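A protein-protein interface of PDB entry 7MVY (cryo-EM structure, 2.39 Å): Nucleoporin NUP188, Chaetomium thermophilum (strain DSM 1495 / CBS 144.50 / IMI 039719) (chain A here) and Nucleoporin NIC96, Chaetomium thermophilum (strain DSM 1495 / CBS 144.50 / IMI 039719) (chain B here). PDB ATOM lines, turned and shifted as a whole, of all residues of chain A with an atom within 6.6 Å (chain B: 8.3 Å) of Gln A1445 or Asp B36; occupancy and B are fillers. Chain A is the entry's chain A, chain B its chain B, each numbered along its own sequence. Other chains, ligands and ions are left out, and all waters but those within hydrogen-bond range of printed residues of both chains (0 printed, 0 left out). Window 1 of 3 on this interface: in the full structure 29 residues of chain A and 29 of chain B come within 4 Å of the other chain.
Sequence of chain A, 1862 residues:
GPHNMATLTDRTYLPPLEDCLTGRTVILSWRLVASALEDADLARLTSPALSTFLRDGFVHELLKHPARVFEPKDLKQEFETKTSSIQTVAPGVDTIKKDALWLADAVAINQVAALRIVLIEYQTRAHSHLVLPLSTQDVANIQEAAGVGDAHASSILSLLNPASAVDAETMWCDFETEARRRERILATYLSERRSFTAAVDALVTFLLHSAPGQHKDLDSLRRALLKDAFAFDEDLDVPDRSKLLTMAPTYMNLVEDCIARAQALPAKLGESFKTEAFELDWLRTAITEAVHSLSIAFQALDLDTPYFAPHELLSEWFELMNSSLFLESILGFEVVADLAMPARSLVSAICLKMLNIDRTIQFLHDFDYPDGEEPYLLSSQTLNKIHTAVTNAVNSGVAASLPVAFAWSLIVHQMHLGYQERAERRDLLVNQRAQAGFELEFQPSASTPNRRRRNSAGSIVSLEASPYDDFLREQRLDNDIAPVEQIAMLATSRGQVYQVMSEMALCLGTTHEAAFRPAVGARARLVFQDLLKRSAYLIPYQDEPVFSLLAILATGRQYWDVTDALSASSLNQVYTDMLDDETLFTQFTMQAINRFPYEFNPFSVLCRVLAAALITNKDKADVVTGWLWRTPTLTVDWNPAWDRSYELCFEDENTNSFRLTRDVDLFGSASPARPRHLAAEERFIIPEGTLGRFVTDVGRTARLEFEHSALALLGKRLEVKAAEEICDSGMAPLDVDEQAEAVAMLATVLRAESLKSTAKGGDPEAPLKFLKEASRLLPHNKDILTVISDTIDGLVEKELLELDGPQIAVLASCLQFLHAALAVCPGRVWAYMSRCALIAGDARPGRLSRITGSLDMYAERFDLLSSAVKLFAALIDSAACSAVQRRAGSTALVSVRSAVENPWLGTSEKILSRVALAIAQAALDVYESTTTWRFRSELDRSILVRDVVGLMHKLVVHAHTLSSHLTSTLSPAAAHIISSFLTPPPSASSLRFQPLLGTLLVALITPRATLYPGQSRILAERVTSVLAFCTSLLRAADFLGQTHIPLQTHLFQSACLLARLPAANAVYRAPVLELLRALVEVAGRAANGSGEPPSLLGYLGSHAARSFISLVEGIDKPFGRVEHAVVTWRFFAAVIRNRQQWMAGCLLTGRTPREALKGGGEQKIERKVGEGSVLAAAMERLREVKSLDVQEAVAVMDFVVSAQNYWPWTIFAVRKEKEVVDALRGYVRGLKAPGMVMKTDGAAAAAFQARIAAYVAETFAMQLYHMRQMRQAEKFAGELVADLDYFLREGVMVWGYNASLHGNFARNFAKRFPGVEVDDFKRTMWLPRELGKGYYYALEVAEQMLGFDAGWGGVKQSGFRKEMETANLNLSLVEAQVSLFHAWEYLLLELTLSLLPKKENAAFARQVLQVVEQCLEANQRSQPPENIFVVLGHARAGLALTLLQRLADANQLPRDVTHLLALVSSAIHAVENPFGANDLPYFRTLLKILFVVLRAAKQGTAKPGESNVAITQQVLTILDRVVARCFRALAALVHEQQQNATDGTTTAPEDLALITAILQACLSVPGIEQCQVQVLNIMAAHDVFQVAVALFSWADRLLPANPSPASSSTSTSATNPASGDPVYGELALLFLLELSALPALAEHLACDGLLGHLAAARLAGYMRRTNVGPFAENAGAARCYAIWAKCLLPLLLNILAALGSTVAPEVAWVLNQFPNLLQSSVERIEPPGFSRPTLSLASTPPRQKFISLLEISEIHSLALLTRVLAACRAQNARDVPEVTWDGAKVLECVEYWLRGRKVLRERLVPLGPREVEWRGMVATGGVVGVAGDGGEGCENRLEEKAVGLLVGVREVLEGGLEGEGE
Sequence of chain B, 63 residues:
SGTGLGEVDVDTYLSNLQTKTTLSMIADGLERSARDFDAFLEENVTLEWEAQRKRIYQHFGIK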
ATOM      1  N   ALA A1440       5.839 -14.873 -16.152  1.00  0.00           N
ATOM      2  CA  ALA A1440       5.327 -15.922 -17.023  1.00  0.00           C
ATOM      3  C   ALA A1440       5.954 -17.269 -16.696  1.00  0.00           C
ATOM      4  O   ALA A1440       5.297 -18.308 -16.832  1.00  0.00           O
ATOM      5  CB  ALA A1440       5.581 -15.559 -18.487  1.00  0.00           C
ATOM      6  N   LEU A1441       7.215 -17.275 -16.261  1.00  0.00           N
ATOM      7  CA  LEU A1441       7.864 -18.526 -15.886  1.00  0.00           C
ATOM      8  C   LEU A1441       7.076 -19.235 -14.790  1.00  0.00           C
ATOM      9  O   LEU A1441       6.679 -20.396 -14.940  1.00  0.00           O
ATOM     10  CB  LEU A1441       9.300 -18.249 -15.435  1.00  0.00           C
ATOM     11  CG  LEU A1441      10.263 -19.438 -15.356  1.00  0.00           C
ATOM     12  CD1 LEU A1441      11.674 -18.939 -15.107  1.00  0.00           C
ATOM     13  CD2 LEU A1441       9.856 -20.434 -14.277  1.00  0.00           C
ATOM     14  N   THR A1442       6.841 -18.542 -13.674  1.00  0.00           N
ATOM     15  CA  THR A1442       6.119 -19.156 -12.564  1.00  0.00           C
ATOM     16  C   THR A1442       4.667 -19.436 -12.929  1.00  0.00           C
ATOM     17  O   THR A1442       4.096 -20.427 -12.460  1.00  0.00           O
ATOM     18  CB  THR A1442       6.194 -18.270 -11.317  1.00  0.00           C
ATOM     19  OG1 THR A1442       5.549 -18.931 -10.219  1.00  0.00           O
ATOM     20  CG2 THR A1442       5.525 -16.920 -11.550  1.00  0.00           C
ATOM     21  N   LEU A1443       4.054 -18.591 -13.763  1.00  0.00           N
ATOM     22  CA  LEU A1443       2.691 -18.872 -14.204  1.00  0.00           C
ATOM     23  C   LEU A1443       2.624 -20.204 -14.941  1.00  0.00           C
ATOM     24  O   LEU A1443       1.788 -21.061 -14.628  1.00  0.00           O
ATOM     25  CB  LEU A1443       2.175 -17.741 -15.095  1.00  0.00           C
ATOM     26  CG  LEU A1443       1.860 -16.400 -14.429  1.00  0.00           C
ATOM     27  CD1 LEU A1443       1.256 -15.449 -15.451  1.00  0.00           C
ATOM     28  CD2 LEU A1443       0.932 -16.563 -13.234  1.00  0.00           C
ATOM     29  N   LEU A1444       3.499 -20.393 -15.932  1.00  0.00           N
ATOM     30  CA  LEU A1444       3.511 -21.647 -16.675  1.00  0.00           C
ATOM     31  C   LEU A1444       3.869 -22.818 -15.769  1.00  0.00           C
ATOM     32  O   LEU A1444       3.310 -23.911 -15.908  1.00  0.00           O
ATOM     33  CB  LEU A1444       4.491 -21.554 -17.844  1.00  0.00           C
ATOM     34  CG  LEU A1444       4.161 -20.508 -18.914  1.00  0.00           C
ATOM     35  CD1 LEU A1444       5.263 -20.451 -19.961  1.00  0.00           C
ATOM     36  CD2 LEU A1444       2.818 -20.803 -19.566  1.00  0.00           C
ATOM     37  N   GLN A1445       4.793 -22.607 -14.829  1.00  0.00           N
ATOM     38  CA  GLN A1445       5.160 -23.674 -13.904  1.00  0.00           C
ATOM     39  C   GLN A1445       3.952 -24.137 -13.099  1.00  0.00           C
ATOM     40  O   GLN A1445       3.681 -25.339 -12.993  1.00  0.00           O
ATOM     41  CB  GLN A1445       6.277 -23.197 -12.975  1.00  0.00           C
ATOM     42  CG  GLN A1445       6.741 -24.238 -11.968  1.00  0.00           C
ATOM     43  CD  GLN A1445       7.865 -23.732 -11.084  1.00  0.00           C
ATOM     44  OE1 GLN A1445       8.392 -22.640 -11.294  1.00  0.00           O
ATOM     45  NE2 GLN A1445       8.238 -24.526 -10.087  1.00  0.00           N
ATOM     46  N   ARG A1446       3.207 -23.190 -12.524  1.00  0.00           N
ATOM     47  CA  ARG A1446       2.058 -23.555 -11.702  1.00  0.00           C
ATOM     48  C   ARG A1446       0.938 -24.152 -12.548  1.00  0.00           C
ATOM     49  O   ARG A1446       0.259 -25.089 -12.113  1.00  0.00           O
ATOM     50  CB  ARG A1446       1.562 -22.336 -10.927  1.00  0.00           C
ATOM     51  CG  ARG A1446       2.573 -21.801  -9.924  1.00  0.00           C
ATOM     52  CD  ARG A1446       2.024 -20.614  -9.153  1.00  0.00           C
ATOM     53  NE  ARG A1446       3.003 -20.067  -8.216  1.00  0.00           N
ATOM     54  CZ  ARG A1446       3.206 -20.525  -6.982  1.00  0.00           C
ATOM     55  NH1 ARG A1446       2.502 -21.551  -6.520  1.00  0.00           N
ATOM     56  NH2 ARG A1446       4.120 -19.957  -6.210  1.00  0.00           N
ATOM     57  N   LEU A1447       0.733 -23.631 -13.761  1.00  0.00           N
ATOM     58  CA  LEU A1447      -0.301 -24.192 -14.625  1.00  0.00           C
ATOM     59  C   LEU A1447       0.047 -25.607 -15.067  1.00  0.00           C
ATOM     60  O   LEU A1447      -0.853 -26.435 -15.253  1.00  0.00           O
ATOM     61  CB  LEU A1447      -0.520 -23.292 -15.841  1.00  0.00           C
ATOM     62  CG  LEU A1447      -1.603 -22.219 -15.684  1.00  0.00           C
ATOM     63  CD1 LEU A1447      -1.235 -21.202 -14.613  1.00  0.00           C
ATOM     64  CD2 LEU A1447      -1.864 -21.525 -17.012  1.00  0.00           C
ATOM     65  N   ALA A1448       1.337 -25.907 -15.239  1.00  0.00           N
ATOM     66  CA  ALA A1448       1.738 -27.274 -15.551  1.00  0.00           C
ATOM     67  C   ALA A1448       1.602 -28.173 -14.329  1.00  0.00           C
ATOM     68  O   ALA A1448       1.211 -29.339 -14.450  1.00  0.00           O
ATOM     69  CB  ALA A1448       3.174 -27.292 -16.074  1.00  0.00           C
ATOM     70  N   ASP A1449       1.920 -27.646 -13.144  1.00  0.00           N
ATOM     71  CA  ASP A1449       1.686 -28.403 -11.919  1.00  0.00           C
ATOM     72  C   ASP A1449       0.211 -28.750 -11.772  1.00  0.00           C
ATOM     73  O   ASP A1449      -0.137 -29.828 -11.276  1.00  0.00           O
ATOM     74  CB  ASP A1449       2.171 -27.606 -10.707  1.00  0.00           C
ATOM     75  CG  ASP A1449       3.651 -27.284 -10.775  1.00  0.00           C
ATOM     76  OD1 ASP A1449       4.292 -27.641 -11.786  1.00  0.00           O
ATOM     77  OD2 ASP A1449       4.173 -26.676  -9.818  1.00  0.00           O
ATOM     78  N   ALA A1450      -0.672 -27.845 -12.198  1.00  0.00           N
ATOM     79  CA  ALA A1450      -2.104 -28.114 -12.177  1.00  0.00           C
ATOM     80  C   ALA A1450      -2.566 -28.907 -13.392  1.00  0.00           C
ATOM     81  O   ALA A1450      -3.612 -29.563 -13.326  1.00  0.00           O
ATOM     82  CB  ALA A1450      -2.886 -26.802 -12.096  1.00  0.00           C
ATOM     83  N   VAL A1492       9.485 -24.706 -20.132  1.00  0.00           N
ATOM     84  CA  VAL A1492       8.119 -24.986 -19.695  1.00  0.00           C
ATOM     85  C   VAL A1492       7.162 -24.958 -20.881  1.00  0.00           C
ATOM     86  O   VAL A1492       6.195 -25.729 -20.926  1.00  0.00           O
ATOM     87  CB  VAL A1492       7.685 -24.000 -18.590  1.00  0.00           C
ATOM     88  CG1 VAL A1492       8.543 -24.190 -17.347  1.00  0.00           C
ATOM     89  CG2 VAL A1492       7.761 -22.563 -19.077  1.00  0.00           C
ATOM     90  N   ARG A1495       7.553 -28.168 -22.756  1.00  0.00           N
ATOM     91  CA  ARG A1495       7.001 -29.240 -21.936  1.00  0.00           C
ATOM     92  C   ARG A1495       5.481 -29.271 -22.039  1.00  0.00           C
ATOM     93  O   ARG A1495       4.882 -30.337 -22.226  1.00  0.00           O
ATOM     94  CB  ARG A1495       7.438 -29.069 -20.480  1.00  0.00           C
ATOM     95  CG  ARG A1495       6.982 -30.199 -19.569  1.00  0.00           C
ATOM     96  CD  ARG A1495       7.410 -29.970 -18.131  1.00  0.00           C
ATOM     97  NE  ARG A1495       6.994 -31.065 -17.259  1.00  0.00           N
ATOM     98  CZ  ARG A1495       5.783 -31.179 -16.720  1.00  0.00           C
ATOM     99  NH1 ARG A1495       4.850 -30.266 -16.960  1.00  0.00           N
ATOM    100  NH2 ARG A1495       5.501 -32.214 -15.940  1.00  0.00           N
ATOM    101  N   GLU A1811      10.511 -31.010  -1.691  1.00  0.00           N
ATOM    102  CA  GLU A1811       9.378 -30.114  -1.873  1.00  0.00           C
ATOM    103  C   GLU A1811       8.076 -30.847  -2.165  1.00  0.00           C
ATOM    104  O   GLU A1811       7.037 -30.193  -2.314  1.00  0.00           O
ATOM    105  CB  GLU A1811       9.662 -29.119  -3.010  1.00  0.00           C
ATOM    106  CG  GLU A1811      10.783 -28.130  -2.716  1.00  0.00           C
ATOM    107  CD  GLU A1811      12.156 -28.773  -2.720  1.00  0.00           C
ATOM    108  OE1 GLU A1811      12.250 -29.979  -3.037  1.00  0.00           O
ATOM    109  OE2 GLU A1811      13.143 -28.074  -2.406  1.00  0.00           O
ATOM    110  N   GLY B  29       7.026 -15.920  -2.125  1.00  0.00           N
ATOM    111  CA  GLY B  29       6.483 -16.804  -3.142  1.00  0.00           C
ATOM    112  C   GLY B  29       7.448 -17.030  -4.289  1.00  0.00           C
ATOM    113  O   GLY B  29       7.540 -18.136  -4.826  1.00  0.00           O
ATOM    114  N   LEU B  30       8.182 -15.986  -4.679  1.00  0.00           N
ATOM    115  CA  LEU B  30       9.174 -16.133  -5.738  1.00  0.00           C
ATOM    116  C   LEU B  30      10.251 -17.133  -5.337  1.00  0.00           C
ATOM    117  O   LEU B  30      10.621 -18.015  -6.122  1.00  0.00           O
ATOM    118  CB  LEU B  30       9.796 -14.774  -6.064  1.00  0.00           C
ATOM    119  CG  LEU B  30       8.834 -13.698  -6.573  1.00  0.00           C
ATOM    120  CD1 LEU B  30       9.545 -12.358  -6.681  1.00  0.00           C
ATOM    121  CD2 LEU B  30       8.237 -14.095  -7.915  1.00  0.00           C
ATOM    122  N   GLU B  31      10.770 -17.009  -4.113  1.00  0.00           N
ATOM    123  CA  GLU B  31      11.788 -17.942  -3.645  1.00  0.00           C
ATOM    124  C   GLU B  31      11.235 -19.359  -3.555  1.00  0.00           C
ATOM    125  O   GLU B  31      11.919 -20.325  -3.913  1.00  0.00           O
ATOM    126  CB  GLU B  31      12.328 -17.490  -2.288  1.00  0.00           C
ATOM    127  CG  GLU B  31      12.975 -16.115  -2.306  1.00  0.00           C
ATOM    128  CD  GLU B  31      13.505 -15.702  -0.948  1.00  0.00           C
ATOM    129  OE1 GLU B  31      13.365 -16.490   0.011  1.00  0.00           O
ATOM    130  OE2 GLU B  31      14.060 -14.588  -0.837  1.00  0.00           O
ATOM    131  N   ARG B  32       9.997 -19.504  -3.076  1.00  0.00           N
ATOM    132  CA  ARG B  32       9.401 -20.832  -2.981  1.00  0.00           C
ATOM    133  C   ARG B  32       9.251 -21.465  -4.358  1.00  0.00           C
ATOM    134  O   ARG B  32       9.540 -22.653  -4.539  1.00  0.00           O
ATOM    135  CB  ARG B  32       8.045 -20.750  -2.276  1.00  0.00           C
ATOM    136  CG  ARG B  32       7.360 -22.097  -2.103  1.00  0.00           C
ATOM    137  CD  ARG B  32       6.116 -21.996  -1.231  1.00  0.00           C
ATOM    138  NE  ARG B  32       5.115 -21.088  -1.790  1.00  0.00           N
ATOM    139  CZ  ARG B  32       5.019 -19.793  -1.501  1.00  0.00           C
ATOM    140  NH1 ARG B  32       5.863 -19.224  -0.649  1.00  0.00           N
ATOM    141  NH2 ARG B  32       4.069 -19.060  -2.066  1.00  0.00           N
ATOM    142  N   SER B  33       8.808 -20.684  -5.346  1.00  0.00           N
ATOM    143  CA  SER B  33       8.680 -21.209  -6.701  1.00  0.00           C
ATOM    144  C   SER B  33      10.043 -21.569  -7.281  1.00  0.00           C
ATOM    145  O   SER B  33      10.185 -22.596  -7.954  1.00  0.00           O
ATOM    146  CB  SER B  33       7.970 -20.191  -7.592  1.00  0.00           C
ATOM    147  OG  SER B  33       7.831 -20.681  -8.915  1.00  0.00           O
ATOM    148  N   ALA B  34      11.057 -20.737  -7.030  1.00  0.00           N
ATOM    149  CA  ALA B  34      12.391 -21.030  -7.544  1.00  0.00           C
ATOM    150  C   ALA B  34      12.953 -22.299  -6.917  1.00  0.00           C
ATOM    151  O   ALA B  34      13.667 -23.063  -7.578  1.00  0.00           O
ATOM    152  CB  ALA B  34      13.322 -19.846  -7.287  1.00  0.00           C
ATOM    153  N   ARG B  35      12.644 -22.541  -5.642  1.00  0.00           N
ATOM    154  CA  ARG B  35      13.126 -23.747  -4.979  1.00  0.00           C
ATOM    155  C   ARG B  35      12.343 -24.984  -5.401  1.00  0.00           C
ATOM    156  O   ARG B  35      12.909 -26.082  -5.448  1.00  0.00           O
ATOM    157  CB  ARG B  35      13.050 -23.576  -3.460  1.00  0.00           C
ATOM    158  CG  ARG B  35      14.016 -22.540  -2.907  1.00  0.00           C
ATOM    159  CD  ARG B  35      13.861 -22.381  -1.404  1.00  0.00           C
ATOM    160  NE  ARG B  35      14.776 -21.379  -0.863  1.00  0.00           N
ATOM    161  CZ  ARG B  35      14.845 -21.041   0.421  1.00  0.00           C
ATOM    162  NH1 ARG B  35      14.052 -21.624   1.311  1.00  0.00           N
ATOM    163  NH2 ARG B  35      15.710 -20.118   0.817  1.00  0.00           N
ATOM    164  N   ASP B  36      11.053 -24.831  -5.709  1.00  0.00           N
ATOM    165  CA  ASP B  36      10.253 -25.962  -6.162  1.00  0.00           C
ATOM    166  C   ASP B  36      10.488 -26.296  -7.628  1.00  0.00           C
ATOM    167  O   ASP B  36      10.204 -27.424  -8.046  1.00  0.00           O
ATOM    168  CB  ASP B  36       8.765 -25.675  -5.937  1.00  0.00           C
ATOM    169  CG  ASP B  36       8.437 -25.411  -4.481  1.00  0.00           C
ATOM    170  OD1 ASP B  36       9.368 -25.411  -3.649  1.00  0.00           O
ATOM    171  OD2 ASP B  36       7.245 -25.202  -4.168  1.00  0.00           O
ATOM    172  N   PHE B  37      10.989 -25.340  -8.418  1.00  0.00           N
ATOM    173  CA  PHE B  37      11.277 -25.621  -9.819  1.00  0.00           C
ATOM    174  C   PHE B  37      12.330 -26.711  -9.965  1.00  0.00           C
ATOM    175  O   PHE B  37      12.282 -27.494 -10.918  1.00  0.00           O
ATOM    176  CB  PHE B  37      11.733 -24.343 -10.525  1.00  0.00           C
ATOM    177  CG  PHE B  37      11.969 -24.517 -11.999  1.00  0.00           C
ATOM    178  CD1 PHE B  37      10.926 -24.389 -12.900  1.00  0.00           C
ATOM    179  CD2 PHE B  37      13.235 -24.803 -12.482  1.00  0.00           C
ATOM    180  CE1 PHE B  37      11.140 -24.547 -14.256  1.00  0.00           C
ATOM    181  CE2 PHE B  37      13.455 -24.961 -13.837  1.00  0.00           C
ATOM    182  CZ  PHE B  37      12.406 -24.833 -14.726  1.00  0.00           C
ATOM    183  N   ASP B  38      13.283 -26.781  -9.034  1.00  0.00           N
ATOM    184  CA  ASP B  38      14.296 -27.831  -9.094  1.00  0.00           C
ATOM    185  C   ASP B  38      13.657 -29.208  -8.966  1.00  0.00           C
ATOM    186  O   ASP B  38      13.910 -30.103  -9.781  1.00  0.00           O
ATOM    187  CB  ASP B  38      15.338 -27.614  -7.996  1.00  0.00           C
ATOM    188  CG  ASP B  38      16.046 -26.279  -8.119  1.00  0.00           C
ATOM    189  OD1 ASP B  38      16.190 -25.783  -9.257  1.00  0.00           O
ATOM    190  OD2 ASP B  38      16.458 -25.724  -7.079  1.00  0.00           O
ATOM    191  N   ALA B  39      12.823 -29.397  -7.939  1.00  0.00           N
ATOM    192  CA  ALA B  39      12.138 -30.673  -7.773  1.00  0.00           C
ATOM    193  C   ALA B  39      11.202 -30.957  -8.939  1.00  0.00           C
ATOM    194  O   ALA B  39      11.047 -32.115  -9.344  1.00  0.00           O
ATOM    195  CB  ALA B  39      11.363 -30.684  -6.456  1.00  0.00           C
ATOM    196  N   PHE B  40      10.575 -29.919  -9.496  1.00  0.00           N
ATOM    197  CA  PHE B  40       9.685 -30.122 -10.635  1.00  0.00           C
ATOM    198  C   PHE B  40      10.462 -30.633 -11.844  1.00  0.00           C
ATOM    199  O   PHE B  40      10.032 -31.574 -12.521  1.00  0.00           O
ATOM    200  CB  PHE B  40       8.956 -28.819 -10.964  1.00  0.00           C
ATOM    201  CG  PHE B  40       7.909 -28.962 -12.032  1.00  0.00           C
ATOM    202  CD1 PHE B  40       6.819 -29.795 -11.845  1.00  0.00           C
ATOM    203  CD2 PHE B  40       8.007 -28.251 -13.217  1.00  0.00           C
ATOM    204  CE1 PHE B  40       5.853 -29.927 -12.824  1.00  0.00           C
ATOM    205  CE2 PHE B  40       7.042 -28.378 -14.199  1.00  0.00           C
ATOM    206  CZ  PHE B  40       5.964 -29.216 -14.002  1.00  0.00           C
ATOM    207  N   LEU B  41      11.618 -30.029 -12.123  1.00  0.00           N
ATOM    208  CA  LEU B  41      12.447 -30.488 -13.232  1.00  0.00           C
ATOM    209  C   LEU B  41      12.980 -31.893 -12.973  1.00  0.00           C
ATOM    210  O   LEU B  41      13.091 -32.704 -13.901  1.00  0.00           O
ATOM    211  CB  LEU B  41      13.596 -29.503 -13.460  1.00  0.00           C
ATOM    212  CG  LEU B  41      14.438 -29.671 -14.729  1.00  0.00           C
ATOM    213  CD1 LEU B  41      15.134 -28.362 -15.068  1.00  0.00           C
ATOM    214  CD2 LEU B  41      15.464 -30.789 -14.584  1.00  0.00           C
ATOM    215  N   GLU B  42      13.318 -32.198 -11.718  1.00  0.00           N
ATOM    216  CA  GLU B  42      13.760 -33.548 -11.381  1.00  0.00           C
ATOM    217  C   GLU B  42      12.664 -34.567 -11.674  1.00  0.00           C
ATOM    218  O   GLU B  42      12.916 -35.611 -12.285  1.00  0.00           O
ATOM    219  CB  GLU B  42      14.178 -33.612  -9.912  1.00  0.00           C
ATOM    220  CG  GLU B  42      15.484 -32.895  -9.608  1.00  0.00           C
ATOM    221  CD  GLU B  42      15.836 -32.925  -8.134  1.00  0.00           C
ATOM    222  OE1 GLU B  42      15.059 -33.507  -7.347  1.00  0.00           O
ATOM    223  OE2 GLU B  42      16.889 -32.367  -7.761  1.00  0.00           O
ATOM    224  N   GLU B  43      11.436 -34.275 -11.241  1.00  0.00           N
ATOM    225  CA  GLU B  43      10.322 -35.174 -11.524  1.00  0.00           C
ATOM    226  C   GLU B  43      10.073 -35.284 -13.023  1.00  0.00           C
ATOM    227  O   GLU B  43       9.734 -36.361 -13.527  1.00  0.00           O
ATOM    228  CB  GLU B  43       9.062 -34.692 -10.805  1.00  0.00           C
ATOM    229  CG  GLU B  43       9.152 -34.745  -9.287  1.00  0.00           C
ATOM    230  CD  GLU B  43       9.233 -36.162  -8.753  1.00  0.00           C
ATOM    231  OE1 GLU B  43       9.058 -37.110  -9.548  1.00  0.00           O
ATOM    232  OE2 GLU B  43       9.473 -36.329  -7.539  1.00  0.00           O
ATOM    233  N   ASN B  44      10.236 -34.179 -13.752  1.00  0.00           N
ATOM    234  CA  ASN B  44      10.052 -34.211 -15.200  1.00  0.00           C
ATOM    235  C   ASN B  44      11.048 -35.158 -15.855  1.00  0.00           C
ATOM    236  O   ASN B  44      10.671 -36.017 -16.659  1.00  0.00           O
ATOM    237  CB  ASN B  44      10.196 -32.803 -15.779  1.00  0.00           C
ATOM    238  CG  ASN B  44       9.164 -31.840 -15.233  1.00  0.00           C
ATOM    239  OD1 ASN B  44       8.074 -32.242 -14.826  1.00  0.00           O
ATOM    240  ND2 ASN B  44       9.501 -30.557 -15.226  1.00  0.00           N
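N of Phe B37 lies close to NE2 of Gln A1445. OG of Ser B33 lies within hydrogen-bond range of OE1 of Gln A1445, at 3.1 Å. The side-chain hydroxyl (OG) of Ser B33 sits at hydrogen-bond distance from the side-chain hydroxyl (OG1) of Thr A1442, at 3.2 Å. The guanidinium group (NH2) of Arg A1495 lies within hydrogen-bond range of the side-chain amide oxygen (OD1) of Asn B44 (2.8 Å).
Of chain B, only Ser B33, Asp B36 and Phe B37 come within 4 Å of Gln A1445. Asp B36 touches just these residues of chain A: Gln A1445 (3.8 Å) and Glu A1811 (3.2 Å). Printed residues of chain B within 4 Å of Glu A1811: Arg B35, Asp B36 and Ala B39. Printed residues of chain A within 4 Å of Phe B40: Ala A1448 (3.97 Å), Asp A1449 (3.0 Å) and Arg A1495 (3.3 Å). The nearest residue of chain A that does not touch Asp B36 is Asp A1449 (6.1 Å). The nearest printed residue of chain B that does not touch Arg A1495 is Glu B43 (6.2 Å).
O of Phe B40 lies close to ND2 of Asn B44, at 2.9 Å. The backbone carbonyl oxygen (O) of Gln A1445 lies close to the side-chain carboxylate (OD1) of Asp A1449, at 2.7 Å. NE of Arg A1446 sits at hydrogen-bond distance from OG1 of Thr A1442.
Hydrophobic or aromatic side chains of chain A that line the printed part of chain B: Ala A1448. Of the 16 printed residues of chain B, 7 touch a printed residue of chain A. Printed residues of chain B that touch a printed residue of chain A: Ser B33, Arg B35, Asp B36, Phe B37, Ala B39, Phe B40 and Asn B44. Hydrophobic or aromatic side chains of chain B that line the printed part of chain A: Phe B37, Ala B39 and Phe B40. Among the printed residues, 11 pairs touch across the chains.
Among the printed residues, pairs that only touch across the chains: Gln A1445 with Asp B36, Ala A1448 with Phe B40, Asp A1449 with Phe B40, Arg A1495 with Phe B40, Glu A1811 with Arg B35, Glu A1811 with Asp B36 and Glu A1811 with Ala B39.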
